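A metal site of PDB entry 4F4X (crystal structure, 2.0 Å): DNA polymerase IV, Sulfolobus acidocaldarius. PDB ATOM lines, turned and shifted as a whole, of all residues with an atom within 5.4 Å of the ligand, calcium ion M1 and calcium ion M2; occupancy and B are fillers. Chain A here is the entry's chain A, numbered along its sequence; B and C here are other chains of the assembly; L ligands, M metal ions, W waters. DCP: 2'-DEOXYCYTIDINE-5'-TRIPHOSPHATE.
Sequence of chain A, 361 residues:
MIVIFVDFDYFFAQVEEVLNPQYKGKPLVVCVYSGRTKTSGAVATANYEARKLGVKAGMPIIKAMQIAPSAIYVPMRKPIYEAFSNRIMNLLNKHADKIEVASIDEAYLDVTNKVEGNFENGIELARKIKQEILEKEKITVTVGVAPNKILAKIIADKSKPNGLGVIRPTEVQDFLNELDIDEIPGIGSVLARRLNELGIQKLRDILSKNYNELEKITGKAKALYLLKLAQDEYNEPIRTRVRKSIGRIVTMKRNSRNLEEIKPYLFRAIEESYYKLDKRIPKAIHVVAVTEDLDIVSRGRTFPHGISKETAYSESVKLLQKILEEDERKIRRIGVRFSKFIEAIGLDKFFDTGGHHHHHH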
ATOM      1  N   ASP A   7      33.482  17.187 -25.300  1.00  0.00           N
ATOM      2  CA  ASP A   7      33.039  18.324 -24.514  1.00  0.00           C
ATOM      3  C   ASP A   7      31.507  18.224 -24.361  1.00  0.00           C
ATOM      4  O   ASP A   7      30.799  18.174 -25.362  1.00  0.00           O
ATOM      5  CB  ASP A   7      33.519  19.566 -25.279  1.00  0.00           C
ATOM      6  CG  ASP A   7      33.173  20.847 -24.617  1.00  0.00           C
ATOM      7  OD1 ASP A   7      34.034  21.736 -24.527  1.00  0.00           O
ATOM      8  OD2 ASP A   7      32.017  21.011 -24.267  1.00  0.00           O
ATOM      9  N   PHE A   8      30.993  18.155 -23.128  1.00  0.00           N
ATOM     10  CA  PHE A   8      29.578  17.840 -22.905  1.00  0.00           C
ATOM     11  C   PHE A   8      28.689  19.027 -23.219  1.00  0.00           C
ATOM     12  O   PHE A   8      28.979  20.095 -22.764  1.00  0.00           O
ATOM     13  CB  PHE A   8      29.308  17.442 -21.452  1.00  0.00           C
ATOM     14  CG  PHE A   8      30.214  16.355 -20.935  1.00  0.00           C
ATOM     15  CD1 PHE A   8      30.444  16.241 -19.577  1.00  0.00           C
ATOM     16  CD2 PHE A   8      30.797  15.438 -21.795  1.00  0.00           C
ATOM     17  CE1 PHE A   8      31.236  15.226 -19.078  1.00  0.00           C
ATOM     18  CE2 PHE A   8      31.636  14.425 -21.297  1.00  0.00           C
ATOM     19  CZ  PHE A   8      31.845  14.328 -19.938  1.00  0.00           C
ATOM     20  N   ASP A   9      27.589  18.871 -23.948  1.00  0.00           N
ATOM     21  CA  ASP A   9      26.786  20.074 -24.281  1.00  0.00           C
ATOM     22  C   ASP A   9      26.045  20.670 -23.079  1.00  0.00           C
ATOM     23  O   ASP A   9      25.459  19.939 -22.282  1.00  0.00           O
ATOM     24  CB  ASP A   9      25.775  19.771 -25.399  1.00  0.00           C
ATOM     25  CG  ASP A   9      26.436  19.267 -26.672  1.00  0.00           C
ATOM     26  OD1 ASP A   9      25.767  18.530 -27.418  1.00  0.00           O
ATOM     27  OD2 ASP A   9      27.617  19.595 -26.936  1.00  0.00           O
ATOM     28  N   TYR A  10      26.063  22.000 -22.979  1.00  0.00           N
ATOM     29  CA  TYR A  10      25.373  22.761 -21.904  1.00  0.00           C
ATOM     30  C   TYR A  10      25.257  21.980 -20.578  1.00  0.00           C
ATOM     31  O   TYR A  10      24.190  21.847 -20.002  1.00  0.00           O
ATOM     32  CB  TYR A  10      24.003  23.340 -22.386  1.00  0.00           C
ATOM     33  CG  TYR A  10      22.938  22.323 -22.800  1.00  0.00           C
ATOM     34  CD1 TYR A  10      21.829  22.082 -21.994  1.00  0.00           C
ATOM     35  CD2 TYR A  10      23.032  21.634 -24.003  1.00  0.00           C
ATOM     36  CE1 TYR A  10      20.820  21.157 -22.364  1.00  0.00           C
ATOM     37  CE2 TYR A  10      22.043  20.701 -24.383  1.00  0.00           C
ATOM     38  CZ  TYR A  10      20.946  20.473 -23.553  1.00  0.00           C
ATOM     39  OH  TYR A  10      19.974  19.572 -23.921  1.00  0.00           O
ATOM     40  N   PHE A  11      26.416  21.500 -20.109  1.00  0.00           N
ATOM     41  CA  PHE A  11      26.479  20.379 -19.167  1.00  0.00           C
ATOM     42  C   PHE A  11      25.515  20.428 -17.981  1.00  0.00           C
ATOM     43  O   PHE A  11      24.656  19.563 -17.855  1.00  0.00           O
ATOM     44  CB  PHE A  11      27.922  20.128 -18.690  1.00  0.00           C
ATOM     45  CG  PHE A  11      28.094  18.838 -17.899  1.00  0.00           C
ATOM     46  CD1 PHE A  11      27.488  17.671 -18.334  1.00  0.00           C
ATOM     47  CD2 PHE A  11      28.865  18.799 -16.751  1.00  0.00           C
ATOM     48  CE1 PHE A  11      27.613  16.471 -17.621  1.00  0.00           C
ATOM     49  CE2 PHE A  11      29.005  17.616 -16.030  1.00  0.00           C
ATOM     50  CZ  PHE A  11      28.378  16.456 -16.455  1.00  0.00           C
ATOM     51  N   PHE A  12      25.657  21.423 -17.101  1.00  0.00           N
ATOM     52  CA  PHE A  12      24.852  21.410 -15.879  1.00  0.00           C
ATOM     53  C   PHE A  12      23.358  21.427 -16.200  1.00  0.00           C
ATOM     54  O   PHE A  12      22.569  20.705 -15.567  1.00  0.00           O
ATOM     55  CB  PHE A  12      25.220  22.550 -14.910  1.00  0.00           C
ATOM     56  CG  PHE A  12      26.642  22.464 -14.355  1.00  0.00           C
ATOM     57  CD1 PHE A  12      27.499  21.432 -14.709  1.00  0.00           C
ATOM     58  CD2 PHE A  12      27.113  23.427 -13.461  1.00  0.00           C
ATOM     59  CE1 PHE A  12      28.814  21.361 -14.203  1.00  0.00           C
ATOM     60  CE2 PHE A  12      28.417  23.354 -12.946  1.00  0.00           C
ATOM     61  CZ  PHE A  12      29.246  22.310 -13.322  1.00  0.00           C
ATOM     62  N   ALA A  13      22.946  22.240 -17.179  1.00  0.00           N
ATOM     63  CA  ALA A  13      21.543  22.303 -17.571  1.00  0.00           C
ATOM     64  C   ALA A  13      21.088  20.998 -18.201  1.00  0.00           C
ATOM     65  O   ALA A  13      19.950  20.575 -17.990  1.00  0.00           O
ATOM     66  CB  ALA A  13      21.269  23.535 -18.565  1.00  0.00           C
ATOM     67  N   VAL A  43      24.462  32.985 -12.896  1.00  0.00           N
ATOM     68  CA  VAL A  43      24.110  31.887 -13.789  1.00  0.00           C
ATOM     69  C   VAL A  43      25.315  30.994 -14.016  1.00  0.00           C
ATOM     70  O   VAL A  43      26.380  31.485 -14.420  1.00  0.00           O
ATOM     71  CB  VAL A  43      23.590  32.420 -15.150  1.00  0.00           C
ATOM     72  CG1 VAL A  43      23.404  31.281 -16.152  1.00  0.00           C
ATOM     73  CG2 VAL A  43      22.289  33.216 -14.957  1.00  0.00           C
ATOM     74  N   ALA A  44      25.165  29.702 -13.719  1.00  0.00           N
ATOM     75  CA  ALA A  44      26.248  28.736 -13.945  1.00  0.00           C
ATOM     76  C   ALA A  44      26.244  28.310 -15.409  1.00  0.00           C
ATOM     77  O   ALA A  44      27.295  28.198 -16.031  1.00  0.00           O
ATOM     78  CB  ALA A  44      26.104  27.493 -13.027  1.00  0.00           C
ATOM     79  N   THR A  45      25.060  28.048 -15.953  1.00  0.00           N
ATOM     80  CA  THR A  45      24.929  27.757 -17.365  1.00  0.00           C
ATOM     81  C   THR A  45      23.461  27.808 -17.787  1.00  0.00           C
ATOM     82  O   THR A  45      22.557  27.810 -16.962  1.00  0.00           O
ATOM     83  CB  THR A  45      25.531  26.410 -17.751  1.00  0.00           C
ATOM     84  OG1 THR A  45      25.753  26.366 -19.171  1.00  0.00           O
ATOM     85  CG2 THR A  45      24.635  25.273 -17.323  1.00  0.00           C
ATOM     86  N   ALA A  46      23.208  27.860 -19.076  1.00  0.00           N
ATOM     87  CA  ALA A  46      21.826  27.906 -19.542  1.00  0.00           C
ATOM     88  C   ALA A  46      21.736  26.987 -20.720  1.00  0.00           C
ATOM     89  O   ALA A  46      22.683  26.894 -21.481  1.00  0.00           O
ATOM     90  CB  ALA A  46      21.469  29.313 -19.949  1.00  0.00           C
ATOM     91  N   TYR A  48      20.447  25.901 -24.512  1.00  0.00           N
ATOM     92  CA  TYR A  48      20.483  26.706 -25.733  1.00  0.00           C
ATOM     93  C   TYR A  48      19.220  27.530 -25.965  1.00  0.00           C
ATOM     94  O   TYR A  48      19.306  28.630 -26.487  1.00  0.00           O
ATOM     95  CB  TYR A  48      20.837  25.844 -26.945  1.00  0.00           C
ATOM     96  CG  TYR A  48      22.322  25.591 -26.997  1.00  0.00           C
ATOM     97  CD1 TYR A  48      23.159  26.363 -27.789  1.00  0.00           C
ATOM     98  CD2 TYR A  48      22.896  24.610 -26.193  1.00  0.00           C
ATOM     99  CE1 TYR A  48      24.532  26.141 -27.820  1.00  0.00           C
ATOM    100  CE2 TYR A  48      24.262  24.389 -26.201  1.00  0.00           C
ATOM    101  CZ  TYR A  48      25.073  25.152 -27.002  1.00  0.00           C
ATOM    102  OH  TYR A  48      26.432  24.911 -27.011  1.00  0.00           O
ATOM    103  N   ARG A  51      19.765  30.586 -24.002  1.00  0.00           N
ATOM    104  CA  ARG A  51      20.844  31.388 -24.580  1.00  0.00           C
ATOM    105  C   ARG A  51      20.305  32.212 -25.737  1.00  0.00           C
ATOM    106  O   ARG A  51      20.776  33.329 -25.988  1.00  0.00           O
ATOM    107  CB  ARG A  51      22.004  30.509 -25.052  1.00  0.00           C
ATOM    108  CG  ARG A  51      22.773  29.856 -23.871  1.00  0.00           C
ATOM    109  CD  ARG A  51      23.915  28.999 -24.360  1.00  0.00           C
ATOM    110  NE  ARG A  51      24.380  28.096 -23.326  1.00  0.00           N
ATOM    111  CZ  ARG A  51      25.461  27.342 -23.415  1.00  0.00           C
ATOM    112  NH1 ARG A  51      26.211  27.377 -24.514  1.00  0.00           N
ATOM    113  NH2 ARG A  51      25.815  26.548 -22.399  1.00  0.00           N
ATOM    114  N   ALA A  57      26.259  32.494 -19.070  1.00  0.00           N
ATOM    115  CA  ALA A  57      27.007  32.064 -17.875  1.00  0.00           C
ATOM    116  C   ALA A  57      27.790  33.237 -17.290  1.00  0.00           C
ATOM    117  O   ALA A  57      28.431  33.991 -18.014  1.00  0.00           O
ATOM    118  CB  ALA A  57      27.968  30.960 -18.233  1.00  0.00           C
ATOM    119  N   GLY A  58      27.714  33.396 -15.966  1.00  0.00           N
ATOM    120  CA  GLY A  58      28.392  34.471 -15.259  1.00  0.00           C
ATOM    121  C   GLY A  58      27.444  35.603 -14.903  1.00  0.00           C
ATOM    122  O   GLY A  58      27.663  36.356 -13.969  1.00  0.00           O
ATOM    123  N   MET A  76      21.924  25.192  -8.629  1.00  0.00           N
ATOM    124  CA  MET A  76      23.009  24.320  -8.994  1.00  0.00           C
ATOM    125  C   MET A  76      23.099  23.165  -7.977  1.00  0.00           C
ATOM    126  O   MET A  76      22.973  23.374  -6.772  1.00  0.00           O
ATOM    127  CB  MET A  76      24.320  25.102  -9.044  1.00  0.00           C
ATOM    128  CG  MET A  76      25.426  24.372  -9.812  1.00  0.00           C
ATOM    129  SD  MET A  76      27.013  25.192  -9.736  1.00  0.00           S
ATOM    130  CE  MET A  76      27.190  25.391  -7.966  1.00  0.00           C
ATOM    131  N   SER A 103      38.621  18.694 -17.188  1.00  0.00           N
ATOM    132  CA  SER A 103      37.706  19.323 -16.241  1.00  0.00           C
ATOM    133  C   SER A 103      36.462  18.410 -16.109  1.00  0.00           C
ATOM    134  O   SER A 103      36.395  17.360 -16.718  1.00  0.00           O
ATOM    135  CB  SER A 103      37.265  20.694 -16.743  1.00  0.00           C
ATOM    136  OG  SER A 103      36.294  20.576 -17.777  1.00  0.00           O
ATOM    137  N   ILE A 104      35.488  18.841 -15.321  1.00  0.00           N
ATOM    138  CA  ILE A 104      34.267  18.080 -15.087  1.00  0.00           C
ATOM    139  C   ILE A 104      33.508  17.887 -16.407  1.00  0.00           C
ATOM    140  O   ILE A 104      32.662  17.007 -16.552  1.00  0.00           O
ATOM    141  CB  ILE A 104      33.388  18.844 -14.059  1.00  0.00           C
ATOM    142  CG1 ILE A 104      32.209  18.032 -13.578  1.00  0.00           C
ATOM    143  CG2 ILE A 104      32.879  20.154 -14.623  1.00  0.00           C
ATOM    144  CD1 ILE A 104      31.327  18.872 -12.677  1.00  0.00           C
ATOM    145  N   ASP A 105      33.854  18.705 -17.385  1.00  0.00           N
ATOM    146  CA  ASP A 105      33.089  18.843 -18.615  1.00  0.00           C
ATOM    147  C   ASP A 105      33.807  18.298 -19.875  1.00  0.00           C
ATOM    148  O   ASP A 105      33.198  18.088 -20.910  1.00  0.00           O
ATOM    149  CB  ASP A 105      32.810  20.325 -18.788  1.00  0.00           C
ATOM    150  CG  ASP A 105      32.085  20.602 -20.027  1.00  0.00           C
ATOM    151  OD1 ASP A 105      32.743  20.657 -21.055  1.00  0.00           O
ATOM    152  OD2 ASP A 105      30.848  20.701 -19.993  1.00  0.00           O
ATOM    153  N   GLU A 106      35.121  18.058 -19.796  1.00  0.00           N
ATOM    154  CA  GLU A 106      35.839  17.726 -21.022  1.00  0.00           C
ATOM    155  C   GLU A 106      37.100  16.901 -20.833  1.00  0.00           C
ATOM    156  O   GLU A 106      37.731  16.924 -19.784  1.00  0.00           O
ATOM    157  CB  GLU A 106      36.162  19.022 -21.800  1.00  0.00           C
ATOM    158  CG  GLU A 106      37.368  19.807 -21.273  1.00  0.00           C
ATOM    159  CD  GLU A 106      37.493  21.170 -21.941  1.00  0.00           C
ATOM    160  OE1 GLU A 106      36.469  21.828 -22.099  1.00  0.00           O
ATOM    161  OE2 GLU A 106      38.600  21.611 -22.349  1.00  0.00           O
ATOM    162  N   LYS A 153      40.214  20.652 -29.916  1.00  0.00           N
ATOM    163  CA  LYS A 153      39.318  21.519 -29.151  1.00  0.00           C
ATOM    164  C   LYS A 153      38.675  22.620 -29.998  1.00  0.00           C
ATOM    165  O   LYS A 153      37.487  22.890 -29.864  1.00  0.00           O
ATOM    166  CB  LYS A 153      40.055  22.125 -27.955  1.00  0.00           C
ATOM    167  CG  LYS A 153      39.194  23.036 -27.102  1.00  0.00           C
ATOM    168  CD  LYS A 153      40.017  23.602 -25.935  1.00  0.00           C
ATOM    169  CE  LYS A 153      39.171  24.430 -24.986  1.00  0.00           C
ATOM    170  NZ  LYS A 153      38.130  23.607 -24.307  1.00  0.00           N
ATOM    171  N   LYS A 160      29.639  22.954 -32.125  1.00  0.00           N
ATOM    172  CA  LYS A 160      28.591  22.888 -31.111  1.00  0.00           C
ATOM    173  C   LYS A 160      27.216  23.358 -31.605  1.00  0.00           C
ATOM    174  O   LYS A 160      27.124  24.285 -32.411  1.00  0.00           O
ATOM    175  CB  LYS A 160      28.994  23.686 -29.867  1.00  0.00           C
ATOM    176  CG  LYS A 160      30.267  23.167 -29.219  1.00  0.00           C
ATOM    177  CD  LYS A 160      30.324  23.536 -27.759  1.00  0.00           C
ATOM    178  CE  LYS A 160      29.402  22.657 -26.972  1.00  0.00           C
ATOM    179  NZ  LYS A 160      30.082  21.571 -26.186  1.00  0.00           N
ATOM    180  P    DG B  13      36.187  30.422 -20.604  1.00  0.00           P
ATOM    181  OP1  DG B  13      37.283  30.287 -21.589  1.00  0.00           O
ATOM    182  OP2  DG B  13      34.900  31.045 -20.927  1.00  0.00           O
ATOM    183  O5'  DG B  13      35.850  28.941 -20.069  1.00  0.00           O
ATOM    184  C5'  DG B  13      36.908  28.144 -19.519  1.00  0.00           C
ATOM    185  C4'  DG B  13      36.435  27.190 -18.429  1.00  0.00           C
ATOM    186  O4'  DG B  13      36.201  27.841 -17.163  1.00  0.00           O
ATOM    187  C3'  DG B  13      35.127  26.446 -18.631  1.00  0.00           C
ATOM    188  O3'  DG B  13      35.324  25.301 -17.863  1.00  0.00           O
ATOM    189  C2'  DG B  13      34.077  27.360 -18.002  1.00  0.00           C
ATOM    190  C1'  DG B  13      34.855  27.689 -16.745  1.00  0.00           C
ATOM    191  N9   DG B  13      34.578  28.966 -16.124  1.00  0.00           N
ATOM    192  C8   DG B  13      34.712  30.206 -16.708  1.00  0.00           C
ATOM    193  N7   DG B  13      34.425  31.188 -15.894  1.00  0.00           N
ATOM    194  C5   DG B  13      34.106  30.537 -14.693  1.00  0.00           C
ATOM    195  C6   DG B  13      33.731  31.070 -13.441  1.00  0.00           C
ATOM    196  O6   DG B  13      33.601  32.271 -13.145  1.00  0.00           O
ATOM    197  N1   DG B  13      33.490  30.067 -12.485  1.00  0.00           N
ATOM    198  C2   DG B  13      33.633  28.713 -12.698  1.00  0.00           C
ATOM    199  N2   DG B  13      33.361  27.897 -11.660  1.00  0.00           N
ATOM    200  N3   DG B  13      33.987  28.211 -13.872  1.00  0.00           N
ATOM    201  C4   DG B  13      34.210  29.168 -14.814  1.00  0.00           C
ATOM    202  P    DC B  14      35.424  23.896 -18.601  1.00  0.00           P
ATOM    203  OP1  DC B  14      34.558  23.975 -19.741  1.00  0.00           O
ATOM    204  OP2  DC B  14      35.101  22.825 -17.607  1.00  0.00           O
ATOM    205  O5'  DC B  14      36.981  23.768 -18.994  1.00  0.00           O
ATOM    206  C5'  DC B  14      37.611  24.228 -20.217  1.00  0.00           C
ATOM    207  C4'  DC B  14      39.131  24.311 -20.041  1.00  0.00           C
ATOM    208  O4'  DC B  14      39.388  25.348 -19.051  1.00  0.00           O
ATOM    209  C3'  DC B  14      39.893  23.069 -19.537  1.00  0.00           C
ATOM    210  O3'  DC B  14      41.171  22.888 -20.178  1.00  0.00           O
ATOM    211  C2'  DC B  14      40.142  23.360 -18.051  1.00  0.00           C
ATOM    212  C1'  DC B  14      40.335  24.873 -18.088  1.00  0.00           C
ATOM    213  N1   DC B  14      40.087  25.516 -16.766  1.00  0.00           N
ATOM    214  C2   DC B  14      41.038  26.390 -16.227  1.00  0.00           C
ATOM    215  O2   DC B  14      42.075  26.610 -16.883  1.00  0.00           O
ATOM    216  N3   DC B  14      40.789  26.955 -15.012  1.00  0.00           N
ATOM    217  C4   DC B  14      39.651  26.678 -14.369  1.00  0.00           C
ATOM    218  N4   DC B  14      39.434  27.271 -13.189  1.00  0.00           N
ATOM    219  C5   DC B  14      38.659  25.809 -14.910  1.00  0.00           C
ATOM    220  C6   DC B  14      38.919  25.248 -16.091  1.00  0.00           C
ATOM    221  P    DG C   5      26.227  37.306  -5.418  1.00  0.00           P
ATOM    222  OP1  DG C   5      25.164  37.503  -4.408  1.00  0.00           O
ATOM    223  OP2  DG C   5      27.578  37.833  -5.205  1.00  0.00           O
ATOM    224  O5'  DG C   5      26.262  35.728  -5.679  1.00  0.00           O
ATOM    225  C5'  DG C   5      26.940  35.199  -6.803  1.00  0.00           C
ATOM    226  C4'  DG C   5      27.027  33.716  -6.544  1.00  0.00           C
ATOM    227  O4'  DG C   5      27.451  32.997  -7.720  1.00  0.00           O
ATOM    228  C3'  DG C   5      28.105  33.449  -5.489  1.00  0.00           C
ATOM    229  O3'  DG C   5      27.706  32.297  -4.810  1.00  0.00           O
ATOM    230  C2'  DG C   5      29.357  33.305  -6.339  1.00  0.00           C
ATOM    231  C1'  DG C   5      28.799  32.562  -7.552  1.00  0.00           C
ATOM    232  N9   DG C   5      29.310  32.853  -8.878  1.00  0.00           N
ATOM    233  C8   DG C   5      29.613  34.088  -9.396  1.00  0.00           C
ATOM    234  N7   DG C   5      30.014  34.018 -10.637  1.00  0.00           N
ATOM    235  C5   DG C   5      29.944  32.670 -10.974  1.00  0.00           C
ATOM    236  C6   DG C   5      30.219  31.990 -12.191  1.00  0.00           C
ATOM    237  O6   DG C   5      30.616  32.465 -13.265  1.00  0.00           O
ATOM    238  N1   DG C   5      29.993  30.616 -12.104  1.00  0.00           N
ATOM    239  C2   DG C   5      29.579  29.961 -10.973  1.00  0.00           C
ATOM    240  N2   DG C   5      29.437  28.625 -11.072  1.00  0.00           N
ATOM    241  N3   DG C   5      29.295  30.596  -9.826  1.00  0.00           N
ATOM    242  C4   DG C   5      29.497  31.941  -9.902  1.00  0.00           C
ATOM    243  P    DC C   6      28.555  31.767  -3.553  1.00  0.00           P
ATOM    244  OP1  DC C   6      27.654  30.983  -2.716  1.00  0.00           O
ATOM    245  OP2  DC C   6      29.332  32.920  -2.999  1.00  0.00           O
ATOM    246  O5'  DC C   6      29.621  30.805  -4.203  1.00  0.00           O
ATOM    247  C5'  DC C   6      29.210  29.461  -4.406  1.00  0.00           C
ATOM    248  C4'  DC C   6      30.385  28.826  -5.126  1.00  0.00           C
ATOM    249  O4'  DC C   6      30.632  29.590  -6.324  1.00  0.00           O
ATOM    250  C3'  DC C   6      31.724  28.783  -4.381  1.00  0.00           C
ATOM    251  O3'  DC C   6      32.032  27.418  -4.335  1.00  0.00           O
ATOM    252  C2'  DC C   6      32.691  29.459  -5.330  1.00  0.00           C
ATOM    253  C1'  DC C   6      31.966  29.354  -6.661  1.00  0.00           C
ATOM    254  N1   DC C   6      32.349  30.375  -7.662  1.00  0.00           N
ATOM    255  C2   DC C   6      32.641  29.977  -8.980  1.00  0.00           C
ATOM    256  O2   DC C   6      32.561  28.775  -9.304  1.00  0.00           O
ATOM    257  N3   DC C   6      32.976  30.938  -9.885  1.00  0.00           N
ATOM    258  C4   DC C   6      33.035  32.216  -9.508  1.00  0.00           C
ATOM    259  N4   DC C   6      33.386  33.119 -10.425  1.00  0.00           N
ATOM    260  C5   DC C   6      32.759  32.635  -8.168  1.00  0.00           C
ATOM    261  C6   DC C   6      32.415  31.684  -7.293  1.00  0.00           C
HETATM  262  N1  DCP L   1      30.461  26.873 -15.577  1.00  0.00           N
HETATM  263  C2  DCP L   1      30.260  27.633 -14.488  1.00  0.00           C
HETATM  264  N3  DCP L   1      30.400  28.968 -14.506  1.00  0.00           N
HETATM  265  C4  DCP L   1      30.744  29.592 -15.655  1.00  0.00           C
HETATM  266  C5  DCP L   1      30.935  28.854 -16.813  1.00  0.00           C
HETATM  267  C6  DCP L   1      30.773  27.458 -16.756  1.00  0.00           C
HETATM  268  O2  DCP L   1      29.935  27.021 -13.338  1.00  0.00           O
HETATM  269  N4  DCP L   1      30.869  31.011 -15.696  1.00  0.00           N
HETATM  270  C1' DCP L   1      30.265  25.412 -15.514  1.00  0.00           C
HETATM  271  C2' DCP L   1      28.888  25.091 -15.951  1.00  0.00           C
HETATM  272  C3' DCP L   1      29.054  24.627 -17.364  1.00  0.00           C
HETATM  273  C4' DCP L   1      30.275  23.888 -17.246  1.00  0.00           C
HETATM  274  O4' DCP L   1      31.097  24.759 -16.418  1.00  0.00           O
HETATM  275  O3' DCP L   1      27.980  23.837 -17.834  1.00  0.00           O
HETATM  276  C5' DCP L   1      30.914  23.696 -18.555  1.00  0.00           C
HETATM  277  O5' DCP L   1      31.398  24.852 -19.184  1.00  0.00           O
HETATM  278  PA  DCP L   1      31.230  25.192 -20.700  1.00  0.00           P
HETATM  279  O1A DCP L   1      32.174  26.264 -21.129  1.00  0.00           O
HETATM  280  O2A DCP L   1      31.790  24.121 -21.484  1.00  0.00           O
HETATM  281  O3A DCP L   1      29.773  25.594 -21.127  1.00  0.00           O
HETATM  282  PB  DCP L   1      28.549  24.627 -21.243  1.00  0.00           P
HETATM  283  O1B DCP L   1      28.830  23.227 -20.949  1.00  0.00           O
HETATM  284  O2B DCP L   1      27.536  24.932 -20.193  1.00  0.00           O
HETATM  285  O3B DCP L   1      27.882  24.831 -22.660  1.00  0.00           O
HETATM  286  PG  DCP L   1      28.498  24.476 -24.062  1.00  0.00           P
HETATM  287  O1G DCP L   1      27.546  23.568 -24.806  1.00  0.00           O
HETATM  288  O2G DCP L   1      28.668  25.716 -24.858  1.00  0.00           O
HETATM  289  O3G DCP L   1      29.848  23.762 -24.105  1.00  0.00           O
HETATM  290 CA    CA M   1      34.055  22.832 -21.964  1.00  0.00          CA
HETATM  291 CA    CA M   2      30.602  21.962 -22.374  1.00  0.00          CA
HETATM  292  O   HOH W   1      31.222  25.239 -11.407  1.00  0.00           O
HETATM  293  O   HOH W   2      28.008  27.779 -19.399  1.00  0.00           O
HETATM  294  O   HOH W   3      31.518  32.425 -18.133  1.00  0.00           O
HETATM  295  O   HOH W   4      34.429  24.845 -23.041  1.00  0.00           O
HETATM  296  O   HOH W   5      30.654  28.544 -20.356  1.00  0.00           O
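The side-chain hydroxyl of Thr 45 sits at hydrogen-bond distance from an oxygen (O2B) of the ligand. The guanidinium group (NH1) of Arg 51 is in salt-bridge range of an oxygen (O2G) of the ligand (3.0 Å). The side-chain hydroxyl (OH) of Tyr 48 lies within hydrogen-bond range of an oxygen (O1G) of the ligand, 2.8 Å away. N4 of the ligand lies within hydrogen-bond range of O6 of DG 5 of chain C, at 2.8 Å. N of Tyr 10 sits at hydrogen-bond distance from O1G of the ligand (2.8 Å). The side-chain amino group (NZ) of Lys 160 is in salt-bridge range of an oxygen (O1G) of the ligand. N of Phe 11 sits close to O1B of the ligand, 3.1 Å away. N of Phe 12 lies within hydrogen-bond range of O3' of the ligand, 3.4 Å away.
The side-chain carboxylate of Asp 7 sits close to the side-chain amino group of Lys 160. OE2 of Glu 106 is in salt-bridge range of NZ of Lys 153 (2.8 Å). N of Glu 106 lies within hydrogen-bond range of OG of Ser 103 (3.4 Å). The backbone NH (N) of Asp 105 lies close to the side-chain hydroxyl (OG) of Ser 103 (3.1 Å). NE of Arg 51 lies within hydrogen-bond range of O of Ala 46, at 2.8 Å. The side-chain carboxylate (OD2) of Asp 9 lies within salt-bridge range of the side-chain amino group (NZ) of Lys 160, 3.2 Å away. N2 of DG 13 of chain B sits close to O2 of DC 6 of chain C (2.6 Å). The backbone NH (N) of Gly 58 sits at hydrogen-bond distance from the backbone carbonyl oxygen (O) of Val 43, at 2.8 Å.
The backbone carbonyl oxygen (O) of Ala 44 lies close to a nitrogen (N1) of the ligand. CA of Asp 9 touches O1G of the ligand, at 3.6 Å. Ala 57 touches the ligand. Gly 58 touches the ligand. C5 of DG 13 of chain B touches N4 of the ligand (3.4 Å). Hydrophobic or aromatic side chains within 4 Å of the ligand: Phe 11, Phe 12, Ala 44, Tyr 48 and Ala 57. Within 4 Å of the ligand: Asp 7, Phe 8, Asp 9, Tyr 10, Phe 11, Phe 12, Ala 44, Thr 45, Tyr 48, Arg 51, Ala 57, Gly 58, Asp 105, Lys 160, DG 13 of chain B, DC 14 of chain B and DG 5 of chain C.
Of the 26 residues printed, 4 come within 4 Å of calcium ion M1.
Lys 160 touches calcium ion M2. The nearest printed residue that does not touch calcium ion M2 is Tyr 10 (4.6 Å).
Calcium ion M1 is bound by water W4 (2.3 Å), OP1 of DC 14 of chain B (2.5 Å), the side-chain carboxylate (OE1) of Glu 106 (2.6 Å), an oxygen (O2A) of the ligand (2.6 Å), the side-chain carboxylate (OD1) of Asp 105 (2.7 Å) and the side-chain carboxylate (OD1) of Asp 7 (2.8 Å).
Calcium ion M2 is bound by O of Phe 8, OD2 of Asp 7, O1B of the ligand, O3G of the ligand, O2A of the ligand, OD2 of Asp 105 and OD1 of Asp 105.
Water W3 bridges a nitrogen (N4) of the ligand (2.9 Å) and the backbone carbonyl oxygen (O) of Ala 57 (3.5 Å). Water W1 lies within hydrogen-bond range of an oxygen (O2) of the ligand (2.9 Å) and N2 of DG 13 of chain B (3.4 Å). Water W2 lies within hydrogen-bond range of OG1 of Thr 45 (2.7 Å), O2B of the ligand (3.0 Å) and O of Ala 44 (3.5 Å).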
